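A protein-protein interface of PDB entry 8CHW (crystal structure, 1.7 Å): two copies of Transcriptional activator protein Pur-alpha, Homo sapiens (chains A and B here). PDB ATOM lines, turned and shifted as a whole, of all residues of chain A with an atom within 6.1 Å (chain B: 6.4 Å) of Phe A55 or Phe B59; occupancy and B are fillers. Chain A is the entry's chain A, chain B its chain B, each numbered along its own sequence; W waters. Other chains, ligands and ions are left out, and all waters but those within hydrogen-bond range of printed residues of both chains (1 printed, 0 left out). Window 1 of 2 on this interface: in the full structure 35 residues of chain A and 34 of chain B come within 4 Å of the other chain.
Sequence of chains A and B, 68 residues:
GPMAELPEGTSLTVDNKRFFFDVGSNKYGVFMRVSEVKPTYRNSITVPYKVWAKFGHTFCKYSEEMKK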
ATOM      1  N   PHE A  21      19.156  -4.530  -3.580  1.00  0.00           N
ATOM      2  CA  PHE A  21      19.789  -5.438  -4.559  1.00  0.00           C
ATOM      3  C   PHE A  21      20.915  -4.676  -5.235  1.00  0.00           C
ATOM      4  O   PHE A  21      20.601  -3.639  -5.859  1.00  0.00           O
ATOM      5  CB  PHE A  21      18.739  -5.879  -5.570  1.00  0.00           C
ATOM      6  CG  PHE A  21      17.604  -6.637  -4.935  1.00  0.00           C
ATOM      7  CD1 PHE A  21      16.500  -5.959  -4.417  1.00  0.00           C
ATOM      8  CD2 PHE A  21      17.639  -8.020  -4.853  1.00  0.00           C
ATOM      9  CE1 PHE A  21      15.450  -6.653  -3.840  1.00  0.00           C
ATOM     10  CE2 PHE A  21      16.591  -8.706  -4.253  1.00  0.00           C
ATOM     11  CZ  PHE A  21      15.511  -8.023  -3.744  1.00  0.00           C
ATOM     12  N   MET A  32      25.158 -10.929  -6.589  1.00  0.00           N
ATOM     13  CA  MET A  32      24.067 -10.034  -6.141  1.00  0.00           C
ATOM     14  C   MET A  32      24.205  -9.916  -4.630  1.00  0.00           C
ATOM     15  O   MET A  32      24.209 -10.951  -3.912  1.00  0.00           O
ATOM     16  CB  MET A  32      22.692 -10.600  -6.512  1.00  0.00           C
ATOM     17  CG  MET A  32      21.492  -9.737  -6.082  1.00  0.00           C
ATOM     18  SD  MET A  32      21.515  -8.187  -6.967  1.00  0.00           S
ATOM     19  CE  MET A  32      20.822  -8.768  -8.519  1.00  0.00           C
ATOM     20  N   VAL A  34      22.268  -8.938  -1.465  1.00  0.00           N
ATOM     21  CA  VAL A  34      20.922  -8.627  -0.920  1.00  0.00           C
ATOM     22  C   VAL A  34      21.088  -8.118   0.506  1.00  0.00           C
ATOM     23  O   VAL A  34      21.478  -8.911   1.382  1.00  0.00           O
ATOM     24  CB  VAL A  34      19.955  -9.822  -0.994  1.00  0.00           C
ATOM     25  CG1 VAL A  34      18.550  -9.376  -0.563  1.00  0.00           C
ATOM     26  CG2 VAL A  34      19.934 -10.401  -2.407  1.00  0.00           C
ATOM     27  N   ILE A  45      23.521 -10.918   2.393  1.00  0.00           N
ATOM     28  CA  ILE A  45      24.086 -12.155   1.800  1.00  0.00           C
ATOM     29  C   ILE A  45      24.529 -11.825   0.378  1.00  0.00           C
ATOM     30  O   ILE A  45      24.126 -10.767  -0.145  1.00  0.00           O
ATOM     31  CB  ILE A  45      23.058 -13.290   1.823  1.00  0.00           C
ATOM     32  CG1 ILE A  45      21.816 -12.928   1.006  1.00  0.00           C
ATOM     33  CG2 ILE A  45      22.742 -13.689   3.241  1.00  0.00           C
ATOM     34  CD1 ILE A  45      20.912 -14.103   0.776  1.00  0.00           C
ATOM     35  N   VAL A  47      25.084 -13.625  -3.516  1.00  0.00           N
ATOM     36  CA  VAL A  47      24.560 -14.735  -4.334  1.00  0.00           C
ATOM     37  C   VAL A  47      25.228 -14.697  -5.706  1.00  0.00           C
ATOM     38  O   VAL A  47      25.103 -13.713  -6.440  1.00  0.00           O
ATOM     39  CB  VAL A  47      23.046 -14.615  -4.468  1.00  0.00           C
ATOM     40  CG1 VAL A  47      22.513 -15.862  -5.155  1.00  0.00           C
ATOM     41  CG2 VAL A  47      22.382 -14.378  -3.127  1.00  0.00           C
ATOM     42  N   VAL A  51      23.289 -18.859  -9.749  1.00  0.00           N
ATOM     43  CA  VAL A  51      22.037 -19.297  -9.065  1.00  0.00           C
ATOM     44  C   VAL A  51      20.977 -18.193  -8.990  1.00  0.00           C
ATOM     45  O   VAL A  51      19.953 -18.466  -8.357  1.00  0.00           O
ATOM     46  CB  VAL A  51      22.283 -19.924  -7.681  1.00  0.00           C
ATOM     47  CG1 VAL A  51      22.996 -21.257  -7.793  1.00  0.00           C
ATOM     48  CG2 VAL A  51      23.028 -18.995  -6.740  1.00  0.00           C
ATOM     49  N   TRP A  52      21.095 -17.055  -9.678  1.00  0.00           N
ATOM     50  CA  TRP A  52      20.028 -16.018  -9.601  1.00  0.00           C
ATOM     51  C   TRP A  52      18.675 -16.587 -10.050  1.00  0.00           C
ATOM     52  O   TRP A  52      17.667 -16.348  -9.359  1.00  0.00           O
ATOM     53  CB  TRP A  52      20.349 -14.750 -10.399  1.00  0.00           C
ATOM     54  CG  TRP A  52      21.503 -13.950  -9.892  1.00  0.00           C
ATOM     55  CD1 TRP A  52      22.255 -14.195  -8.777  1.00  0.00           C
ATOM     56  CD2 TRP A  52      22.004 -12.725 -10.453  1.00  0.00           C
ATOM     57  NE1 TRP A  52      23.203 -13.226  -8.628  1.00  0.00           N
ATOM     58  CE2 TRP A  52      23.085 -12.320  -9.649  1.00  0.00           C
ATOM     59  CE3 TRP A  52      21.688 -11.957 -11.576  1.00  0.00           C
ATOM     60  CZ2 TRP A  52      23.855 -11.200  -9.951  1.00  0.00           C
ATOM     61  CZ3 TRP A  52      22.437 -10.845 -11.863  1.00  0.00           C
ATOM     62  CH2 TRP A  52      23.481 -10.442 -11.035  1.00  0.00           C
ATOM     63  N   ALA A  53      18.622 -17.247 -11.201  1.00  0.00           N
ATOM     64  CA  ALA A  53      17.346 -17.770 -11.758  1.00  0.00           C
ATOM     65  C   ALA A  53      16.714 -18.756 -10.762  1.00  0.00           C
ATOM     66  O   ALA A  53      15.528 -18.614 -10.484  1.00  0.00           O
ATOM     67  CB  ALA A  53      17.581 -18.380 -13.130  1.00  0.00           C
ATOM     68  N   LYS A  54      17.492 -19.678 -10.205  1.00  0.00           N
ATOM     69  CA  LYS A  54      17.009 -20.663  -9.195  1.00  0.00           C
ATOM     70  C   LYS A  54      16.550 -19.950  -7.911  1.00  0.00           C
ATOM     71  O   LYS A  54      15.552 -20.394  -7.332  1.00  0.00           O
ATOM     72  CB  LYS A  54      18.104 -21.687  -8.900  1.00  0.00           C
ATOM     73  CG  LYS A  54      18.350 -22.706 -10.000  1.00  0.00           C
ATOM     74  CD  LYS A  54      19.589 -23.508  -9.715  1.00  0.00           C
ATOM     75  CE  LYS A  54      20.076 -24.341 -10.882  1.00  0.00           C
ATOM     76  NZ  LYS A  54      20.010 -25.776 -10.549  1.00  0.00           N
ATOM     77  N   PHE A  55      17.223 -18.881  -7.463  1.00  0.00           N
ATOM     78  CA  PHE A  55      16.722 -18.042  -6.341  1.00  0.00           C
ATOM     79  C   PHE A  55      15.336 -17.484  -6.679  1.00  0.00           C
ATOM     80  O   PHE A  55      14.381 -17.582  -5.866  1.00  0.00           O
ATOM     81  CB  PHE A  55      17.671 -16.875  -6.050  1.00  0.00           C
ATOM     82  CG  PHE A  55      18.584 -17.110  -4.887  1.00  0.00           C
ATOM     83  CD1 PHE A  55      19.492 -18.148  -4.923  1.00  0.00           C
ATOM     84  CD2 PHE A  55      18.486 -16.349  -3.741  1.00  0.00           C
ATOM     85  CE1 PHE A  55      20.342 -18.367  -3.857  1.00  0.00           C
ATOM     86  CE2 PHE A  55      19.321 -16.601  -2.665  1.00  0.00           C
ATOM     87  CZ  PHE A  55      20.241 -17.605  -2.726  1.00  0.00           C
ATOM     88  N   GLY A  56      15.216 -16.900  -7.870  1.00  0.00           N
ATOM     89  CA  GLY A  56      13.949 -16.327  -8.356  1.00  0.00           C
ATOM     90  C   GLY A  56      12.838 -17.363  -8.293  1.00  0.00           C
ATOM     91  O   GLY A  56      11.793 -17.096  -7.720  1.00  0.00           O
ATOM     92  N   HIS A  57      13.082 -18.525  -8.873  1.00  0.00           N
ATOM     93  CA  HIS A  57      12.115 -19.651  -8.946  1.00  0.00           C
ATOM     94  C   HIS A  57      11.740 -20.064  -7.526  1.00  0.00           C
ATOM     95  O   HIS A  57      10.559 -20.279  -7.258  1.00  0.00           O
ATOM     96  CB  HIS A  57      12.706 -20.803  -9.771  1.00  0.00           C
ATOM     97  CG  HIS A  57      13.057 -20.400 -11.164  1.00  0.00           C
ATOM     98  ND1 HIS A  57      13.847 -21.181 -11.996  1.00  0.00           N
ATOM     99  CD2 HIS A  57      12.739 -19.291 -11.877  1.00  0.00           C
ATOM    100  CE1 HIS A  57      13.986 -20.569 -13.162  1.00  0.00           C
ATOM    101  NE2 HIS A  57      13.325 -19.404 -13.111  1.00  0.00           N
ATOM    102  N   THR A  58      12.723 -20.121  -6.634  1.00  0.00           N
ATOM    103  CA  THR A  58      12.517 -20.577  -5.230  1.00  0.00           C
ATOM    104  C   THR A  58      11.511 -19.624  -4.574  1.00  0.00           C
ATOM    105  O   THR A  58      10.520 -20.119  -4.041  1.00  0.00           O
ATOM    106  CB  THR A  58      13.861 -20.710  -4.499  1.00  0.00           C
ATOM    107  OG1 THR A  58      14.582 -21.818  -5.049  1.00  0.00           O
ATOM    108  CG2 THR A  58      13.695 -20.919  -3.018  1.00  0.00           C
ATOM    109  N   PHE A  59      11.730 -18.303  -4.665  1.00  0.00           N
ATOM    110  CA  PHE A  59      10.844 -17.282  -4.061  1.00  0.00           C
ATOM    111  C   PHE A  59       9.427 -17.372  -4.644  1.00  0.00           C
ATOM    112  O   PHE A  59       8.451 -17.366  -3.884  1.00  0.00           O
ATOM    113  CB  PHE A  59      11.428 -15.883  -4.216  1.00  0.00           C
ATOM    114  CG  PHE A  59      12.312 -15.529  -3.055  1.00  0.00           C
ATOM    115  CD1 PHE A  59      11.757 -15.207  -1.826  1.00  0.00           C
ATOM    116  CD2 PHE A  59      13.682 -15.556  -3.182  1.00  0.00           C
ATOM    117  CE1 PHE A  59      12.562 -14.904  -0.736  1.00  0.00           C
ATOM    118  CE2 PHE A  59      14.487 -15.261  -2.094  1.00  0.00           C
ATOM    119  CZ  PHE A  59      13.924 -14.936  -0.879  1.00  0.00           C
ATOM    120  N   CYS A  60       9.310 -17.495  -5.957  1.00  0.00           N
ATOM    121  CA  CYS A  60       7.996 -17.546  -6.636  1.00  0.00           C
ATOM    122  C   CYS A  60       7.230 -18.804  -6.189  1.00  0.00           C
ATOM    123  O   CYS A  60       6.036 -18.683  -5.895  1.00  0.00           O
ATOM    124  CB  CYS A  60       8.198 -17.460  -8.146  1.00  0.00           C
ATOM    125  SG  CYS A  60       8.694 -15.792  -8.646  1.00  0.00           S
ATOM    126  N   LEU B  12      20.233 -24.388  -1.968  1.00  0.00           N
ATOM    127  CA  LEU B  12      20.966 -24.283  -3.240  1.00  0.00           C
ATOM    128  C   LEU B  12      22.446 -24.216  -2.888  1.00  0.00           C
ATOM    129  O   LEU B  12      22.840 -23.337  -2.087  1.00  0.00           O
ATOM    130  CB  LEU B  12      20.506 -23.033  -3.992  1.00  0.00           C
ATOM    131  CG  LEU B  12      19.116 -23.109  -4.605  1.00  0.00           C
ATOM    132  CD1 LEU B  12      18.711 -21.734  -5.109  1.00  0.00           C
ATOM    133  CD2 LEU B  12      19.038 -24.157  -5.712  1.00  0.00           C
ATOM    134  N   PHE B  19      23.178 -22.116   0.384  1.00  0.00           N
ATOM    135  CA  PHE B  19      22.042 -21.238   0.720  1.00  0.00           C
ATOM    136  C   PHE B  19      20.906 -22.098   1.250  1.00  0.00           C
ATOM    137  O   PHE B  19      20.588 -23.068   0.608  1.00  0.00           O
ATOM    138  CB  PHE B  19      21.617 -20.416  -0.488  1.00  0.00           C
ATOM    139  CG  PHE B  19      22.729 -19.547  -1.010  1.00  0.00           C
ATOM    140  CD1 PHE B  19      22.981 -18.300  -0.452  1.00  0.00           C
ATOM    141  CD2 PHE B  19      23.478 -19.956  -2.105  1.00  0.00           C
ATOM    142  CE1 PHE B  19      24.012 -17.507  -0.945  1.00  0.00           C
ATOM    143  CE2 PHE B  19      24.502 -19.159  -2.588  1.00  0.00           C
ATOM    144  CZ  PHE B  19      24.769 -17.936  -2.008  1.00  0.00           C
ATOM    145  N   PHE B  21      16.889 -21.882   2.493  1.00  0.00           N
ATOM    146  CA  PHE B  21      15.572 -21.214   2.566  1.00  0.00           C
ATOM    147  C   PHE B  21      14.739 -21.904   3.652  1.00  0.00           C
ATOM    148  O   PHE B  21      14.421 -23.094   3.484  1.00  0.00           O
ATOM    149  CB  PHE B  21      14.894 -21.315   1.199  1.00  0.00           C
ATOM    150  CG  PHE B  21      15.725 -20.746   0.073  1.00  0.00           C
ATOM    151  CD1 PHE B  21      16.677 -21.514  -0.565  1.00  0.00           C
ATOM    152  CD2 PHE B  21      15.565 -19.422  -0.323  1.00  0.00           C
ATOM    153  CE1 PHE B  21      17.418 -20.986  -1.613  1.00  0.00           C
ATOM    154  CE2 PHE B  21      16.304 -18.903  -1.372  1.00  0.00           C
ATOM    155  CZ  PHE B  21      17.239 -19.679  -2.002  1.00  0.00           C
ATOM    156  N   VAL B  34      16.837 -16.545   4.613  1.00  0.00           N
ATOM    157  CA  VAL B  34      17.823 -16.997   3.606  1.00  0.00           C
ATOM    158  C   VAL B  34      19.191 -16.930   4.262  1.00  0.00           C
ATOM    159  O   VAL B  34      19.667 -15.809   4.597  1.00  0.00           O
ATOM    160  CB  VAL B  34      17.748 -16.142   2.333  1.00  0.00           C
ATOM    161  CG1 VAL B  34      18.614 -16.718   1.239  1.00  0.00           C
ATOM    162  CG2 VAL B  34      16.292 -15.984   1.912  1.00  0.00           C
ATOM    163  N   LYS B  54       7.895 -10.482  -5.437  1.00  0.00           N
ATOM    164  CA  LYS B  54       8.719  -9.361  -5.958  1.00  0.00           C
ATOM    165  C   LYS B  54      10.215  -9.707  -5.885  1.00  0.00           C
ATOM    166  O   LYS B  54      10.956  -9.301  -6.821  1.00  0.00           O
ATOM    167  CB  LYS B  54       8.378  -8.063  -5.230  1.00  0.00           C
ATOM    168  CG  LYS B  54       7.137  -7.358  -5.739  1.00  0.00           C
ATOM    169  CD  LYS B  54       6.778  -6.144  -4.915  1.00  0.00           C
ATOM    170  CE  LYS B  54       5.673  -5.300  -5.514  1.00  0.00           C
ATOM    171  NZ  LYS B  54       4.334  -5.858  -5.200  1.00  0.00           N
ATOM    172  N   PHE B  55      10.658 -10.417  -4.835  1.00  0.00           N
ATOM    173  CA  PHE B  55      12.040 -10.960  -4.746  1.00  0.00           C
ATOM    174  C   PHE B  55      12.315 -11.885  -5.926  1.00  0.00           C
ATOM    175  O   PHE B  55      13.380 -11.763  -6.533  1.00  0.00           O
ATOM    176  CB  PHE B  55      12.294 -11.761  -3.460  1.00  0.00           C
ATOM    177  CG  PHE B  55      13.030 -10.972  -2.411  1.00  0.00           C
ATOM    178  CD1 PHE B  55      12.508  -9.782  -1.949  1.00  0.00           C
ATOM    179  CD2 PHE B  55      14.257 -11.397  -1.926  1.00  0.00           C
ATOM    180  CE1 PHE B  55      13.169  -9.047  -0.987  1.00  0.00           C
ATOM    181  CE2 PHE B  55      14.948 -10.620  -1.016  1.00  0.00           C
ATOM    182  CZ  PHE B  55      14.389  -9.473  -0.526  1.00  0.00           C
ATOM    183  N   GLY B  56      11.399 -12.819  -6.181  1.00  0.00           N
ATOM    184  CA  GLY B  56      11.477 -13.791  -7.278  1.00  0.00           C
ATOM    185  C   GLY B  56      11.606 -13.064  -8.607  1.00  0.00           C
ATOM    186  O   GLY B  56      12.545 -13.391  -9.381  1.00  0.00           O
ATOM    187  N   HIS B  57      10.731 -12.088  -8.850  1.00  0.00           N
ATOM    188  CA  HIS B  57      10.733 -11.292 -10.108  1.00  0.00           C
ATOM    189  C   HIS B  57      12.071 -10.555 -10.236  1.00  0.00           C
ATOM    190  O   HIS B  57      12.604 -10.457 -11.360  1.00  0.00           O
ATOM    191  CB  HIS B  57       9.602 -10.264 -10.180  1.00  0.00           C
ATOM    192  CG  HIS B  57       8.228 -10.782  -9.916  1.00  0.00           C
ATOM    193  ND1 HIS B  57       7.906 -12.136  -9.992  1.00  0.00           N
ATOM    194  CD2 HIS B  57       7.092 -10.125  -9.567  1.00  0.00           C
ATOM    195  CE1 HIS B  57       6.628 -12.292  -9.689  1.00  0.00           C
ATOM    196  NE2 HIS B  57       6.104 -11.062  -9.425  1.00  0.00           N
ATOM    197  N   THR B  58      12.556  -9.982  -9.138  1.00  0.00           N
ATOM    198  CA  THR B  58      13.784  -9.161  -9.134  1.00  0.00           C
ATOM    199  C   THR B  58      14.947 -10.043  -9.593  1.00  0.00           C
ATOM    200  O   THR B  58      15.696  -9.612 -10.529  1.00  0.00           O
ATOM    201  CB  THR B  58      14.001  -8.460  -7.788  1.00  0.00           C
ATOM    202  OG1 THR B  58      12.977  -7.496  -7.525  1.00  0.00           O
ATOM    203  CG2 THR B  58      15.333  -7.742  -7.723  1.00  0.00           C
ATOM    204  N   PHE B  59      15.112 -11.219  -8.984  1.00  0.00           N
ATOM    205  CA  PHE B  59      16.223 -12.145  -9.315  1.00  0.00           C
ATOM    206  C   PHE B  59      16.125 -12.592 -10.775  1.00  0.00           C
ATOM    207  O   PHE B  59      17.136 -12.581 -11.474  1.00  0.00           O
ATOM    208  CB  PHE B  59      16.240 -13.360  -8.393  1.00  0.00           C
ATOM    209  CG  PHE B  59      17.133 -13.147  -7.193  1.00  0.00           C
ATOM    210  CD1 PHE B  59      18.506 -13.222  -7.314  1.00  0.00           C
ATOM    211  CD2 PHE B  59      16.590 -12.800  -5.973  1.00  0.00           C
ATOM    212  CE1 PHE B  59      19.326 -13.011  -6.210  1.00  0.00           C
ATOM    213  CE2 PHE B  59      17.407 -12.557  -4.880  1.00  0.00           C
ATOM    214  CZ  PHE B  59      18.778 -12.687  -4.996  1.00  0.00           C
ATOM    215  N   CYS B  60      14.942 -12.977 -11.224  1.00  0.00           N
ATOM    216  CA  CYS B  60      14.739 -13.438 -12.629  1.00  0.00           C
ATOM    217  C   CYS B  60      15.087 -12.308 -13.596  1.00  0.00           C
ATOM    218  O   CYS B  60      15.853 -12.592 -14.541  1.00  0.00           O
ATOM    219  CB  CYS B  60      13.322 -13.951 -12.841  1.00  0.00           C
ATOM    220  SG  CYS B  60      13.103 -15.552 -12.033  1.00  0.00           S
ATOM    221  N   LYS B  61      14.624 -11.085 -13.337  1.00  0.00           N
ATOM    222  CA  LYS B  61      14.872  -9.926 -14.235  1.00  0.00           C
ATOM    223  C   LYS B  61      16.371  -9.629 -14.298  1.00  0.00           C
ATOM    224  O   LYS B  61      16.892  -9.428 -15.409  1.00  0.00           O
ATOM    225  CB  LYS B  61      14.121  -8.670 -13.788  1.00  0.00           C
ATOM    226  CG  LYS B  61      12.640  -8.660 -14.151  1.00  0.00           C
ATOM    227  CD  LYS B  61      11.988  -7.300 -13.986  1.00  0.00           C
ATOM    228  CE  LYS B  61      11.438  -7.048 -12.597  1.00  0.00           C
ATOM    229  NZ  LYS B  61      10.033  -7.500 -12.489  1.00  0.00           N
ATOM    230  N   TYR B  62      17.055  -9.564 -13.153  1.00  0.00           N
ATOM    231  CA  TYR B  62      18.521  -9.345 -13.152  1.00  0.00           C
ATOM    232  C   TYR B  62      19.223 -10.481 -13.921  1.00  0.00           C
ATOM    233  O   TYR B  62      20.200 -10.184 -14.636  1.00  0.00           O
ATOM    234  CB  TYR B  62      19.066  -9.175 -11.729  1.00  0.00           C
ATOM    235  CG  TYR B  62      18.955  -7.793 -11.117  1.00  0.00           C
ATOM    236  CD1 TYR B  62      19.651  -6.704 -11.626  1.00  0.00           C
ATOM    237  CD2 TYR B  62      18.252  -7.589  -9.929  1.00  0.00           C
ATOM    238  CE1 TYR B  62      19.605  -5.456 -11.015  1.00  0.00           C
ATOM    239  CE2 TYR B  62      18.221  -6.361  -9.290  1.00  0.00           C
ATOM    240  CZ  TYR B  62      18.882  -5.270  -9.841  1.00  0.00           C
ATOM    241  OH  TYR B  62      18.860  -4.068  -9.168  1.00  0.00           O
ATOM    242  N   SER B  63      18.822 -11.739 -13.728  1.00  0.00           N
ATOM    243  CA  SER B  63      19.392 -12.910 -14.440  1.00  0.00           C
ATOM    244  C   SER B  63      19.309 -12.726 -15.976  1.00  0.00           C
ATOM    245  O   SER B  63      20.347 -12.915 -16.652  1.00  0.00           O
ATOM    246  CB  SER B  63      18.712 -14.189 -14.036  1.00  0.00           C
ATOM    247  OG  SER B  63      19.476 -15.305 -14.474  1.00  0.00           O
ATOM    248  N   GLU B  64      18.123 -12.426 -16.493  1.00  0.00           N
ATOM    249  CA  GLU B  64      17.830 -12.208 -17.946  1.00  0.00           C
ATOM    250  C   GLU B  64      18.663 -11.032 -18.481  1.00  0.00           C
ATOM    251  O   GLU B  64      19.304 -11.199 -19.536  1.00  0.00           O
ATOM    252  CB  GLU B  64      16.350 -11.871 -18.168  1.00  0.00           C
ATOM    253  CG  GLU B  64      15.493 -13.047 -18.576  1.00  0.00           C
ATOM    254  CD  GLU B  64      15.788 -13.547 -19.982  1.00  0.00           C
ATOM    255  OE1 GLU B  64      16.500 -14.559 -20.085  1.00  0.00           O
ATOM    256  OE2 GLU B  64      15.327 -12.893 -20.966  1.00  0.00           O
HETATM  257  O   HOH W   1      21.093 -17.076 -13.061  1.00  0.00           O
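The backbone carbonyl oxygen (O) of Lys A54 is in hydrogen-bond range of the side-chain hydroxyl (OG1) of Thr A58 (2.9 Å).
The side-chain sulfur of Cys A60 sits at hydrogen-bond distance from the backbone carbonyl oxygen of Gly A56 (3.5 Å).
OG1 of Thr B58 lies within hydrogen-bond range of O of Lys B54.
The backbone NH (N) of Met A32 is in hydrogen-bond range of the backbone carbonyl oxygen (O) of Val A47 (2.8 Å).
The backbone carbonyl oxygen (O) of Val A47 is in hydrogen-bond range of the indole nitrogen (NE1) of Trp A52, 2.9 Å away.
The backbone carbonyl oxygen (O) of Ile A45 lies within hydrogen-bond range of the backbone NH (N) of Val A34 (2.9 Å).
Among the printed residues, pairs that only touch across the chains: Phe A21 with Phe B55, Phe A21 with Thr B58, Phe A21 with Phe B59, Phe A21 with Tyr B62, Met A32 with Phe B59, Met A32 with Tyr B62, Val A34 with Phe B55, Val A34 with Phe B59, Ile A45 with Val B34, Val A47 with Phe B19, Trp A52 with Phe B59, Trp A52 with Tyr B62, Trp A52 with Ser B63, Ala A53 with Ser B63, Lys A54 with Leu B12, Phe A55 with Leu B12, Phe A55 with Phe B19, Phe A55 with Phe B21, Phe A55 with Val B34, Phe A55 with Phe B59, Gly A56 with Gly B56, Gly A56 with Phe B59, Gly A56 with Cys B60, His A57 with Cys B60, Thr A58 with Phe B21, Phe A59 with Val B34, Phe A59 with Phe B55, Phe A59 with Gly B56, Cys A60 with Gly B56 and Cys A60 with His B57.
Of the printed residues of chain B, Val A47 touches Phe B19 (3.96 Å).
Val A51 touches none of the printed residues of chain B.
Phe A55 touches just these residues of chain B: Leu B12 (3.7 Å), Phe B19 (3.6 Å), Phe B21 (3.7 Å), Val B34 (3.97 Å) and Phe B59 (3.9 Å).
Of the printed residues of chain A, Val B34 touches Ile A45 (3.5 Å), Phe A55 (3.97 Å) and Phe A59 (3.8 Å).
Printed residues of chain A within 4 Å of Phe B59: Phe A21 (3.99 Å), Met A32 (3.9 Å), Val A34 (3.6 Å), Trp A52 (3.4 Å), Phe A55 (3.9 Å) and Gly A56 (3.7 Å).
The nearest residue of chain B that does not touch Phe A55 is Gly B56 (5.0 Å).
The nearest printed residue of chain A that does not touch Phe B59 is Val A47 (4.4 Å).
The nearest printed residue of chain A that does not touch Ser B63 is Met A32 (6.3 Å).
Printed residues of chain A that touch a printed residue of chain B: Phe A21, Met A32, Val A34, Ile A45, Val A47, Trp A52, Ala A53, Lys A54, Phe A55, Gly A56, His A57, Thr A58, Phe A59 and Cys A60.
Hydrophobic or aromatic side chains of chain A within 4 Å of the printed part of chain B: Phe A21, Met A32, Val A34, Ile A45, Trp A52, Ala A53, Phe A55, His A57 and Phe A59.
Printed residues of chain B that touch a printed residue of chain A: Leu B12, Phe B19, Phe B21, Val B34, Phe B55, Gly B56, His B57, Thr B58, Phe B59, Cys B60, Tyr B62 and Ser B63.
Hydrophobic or aromatic side chains of chain B within 4 Å of the printed part of chain A: Leu B12, Phe B19, Phe B21, Val B34, Phe B55, His B57, Phe B59 and Tyr B62.
Among the printed residues, 30 pairs touch across the chains.
Among the printed residues, no Asp or Glu carboxylate lies within 4 Å of a Lys or Arg side-chain nitrogen of the other chain.
Phe A21 touches Thr B58, and with the chains exchanged Thr A58 touches Phe B21.
Phe A55 touches Phe B59, and with the chains exchanged Phe A59 touches Phe B55.
Gly A56 touches its own counterpart, Gly B56.
Gly A56 touches Cys B60, and with the chains exchanged Cys A60 touches Gly B56.
Of the 30 pairs that touch across the chains among the printed residues, 17 have their exchanged pair printed and touching as well.
Water W1 lies within hydrogen-bond range of the side-chain hydroxyl of Ser B63 (2.8 Å), the backbone NH of Ala A53 (3.1 Å) and the backbone NH of Trp A52 (3.4 Å).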
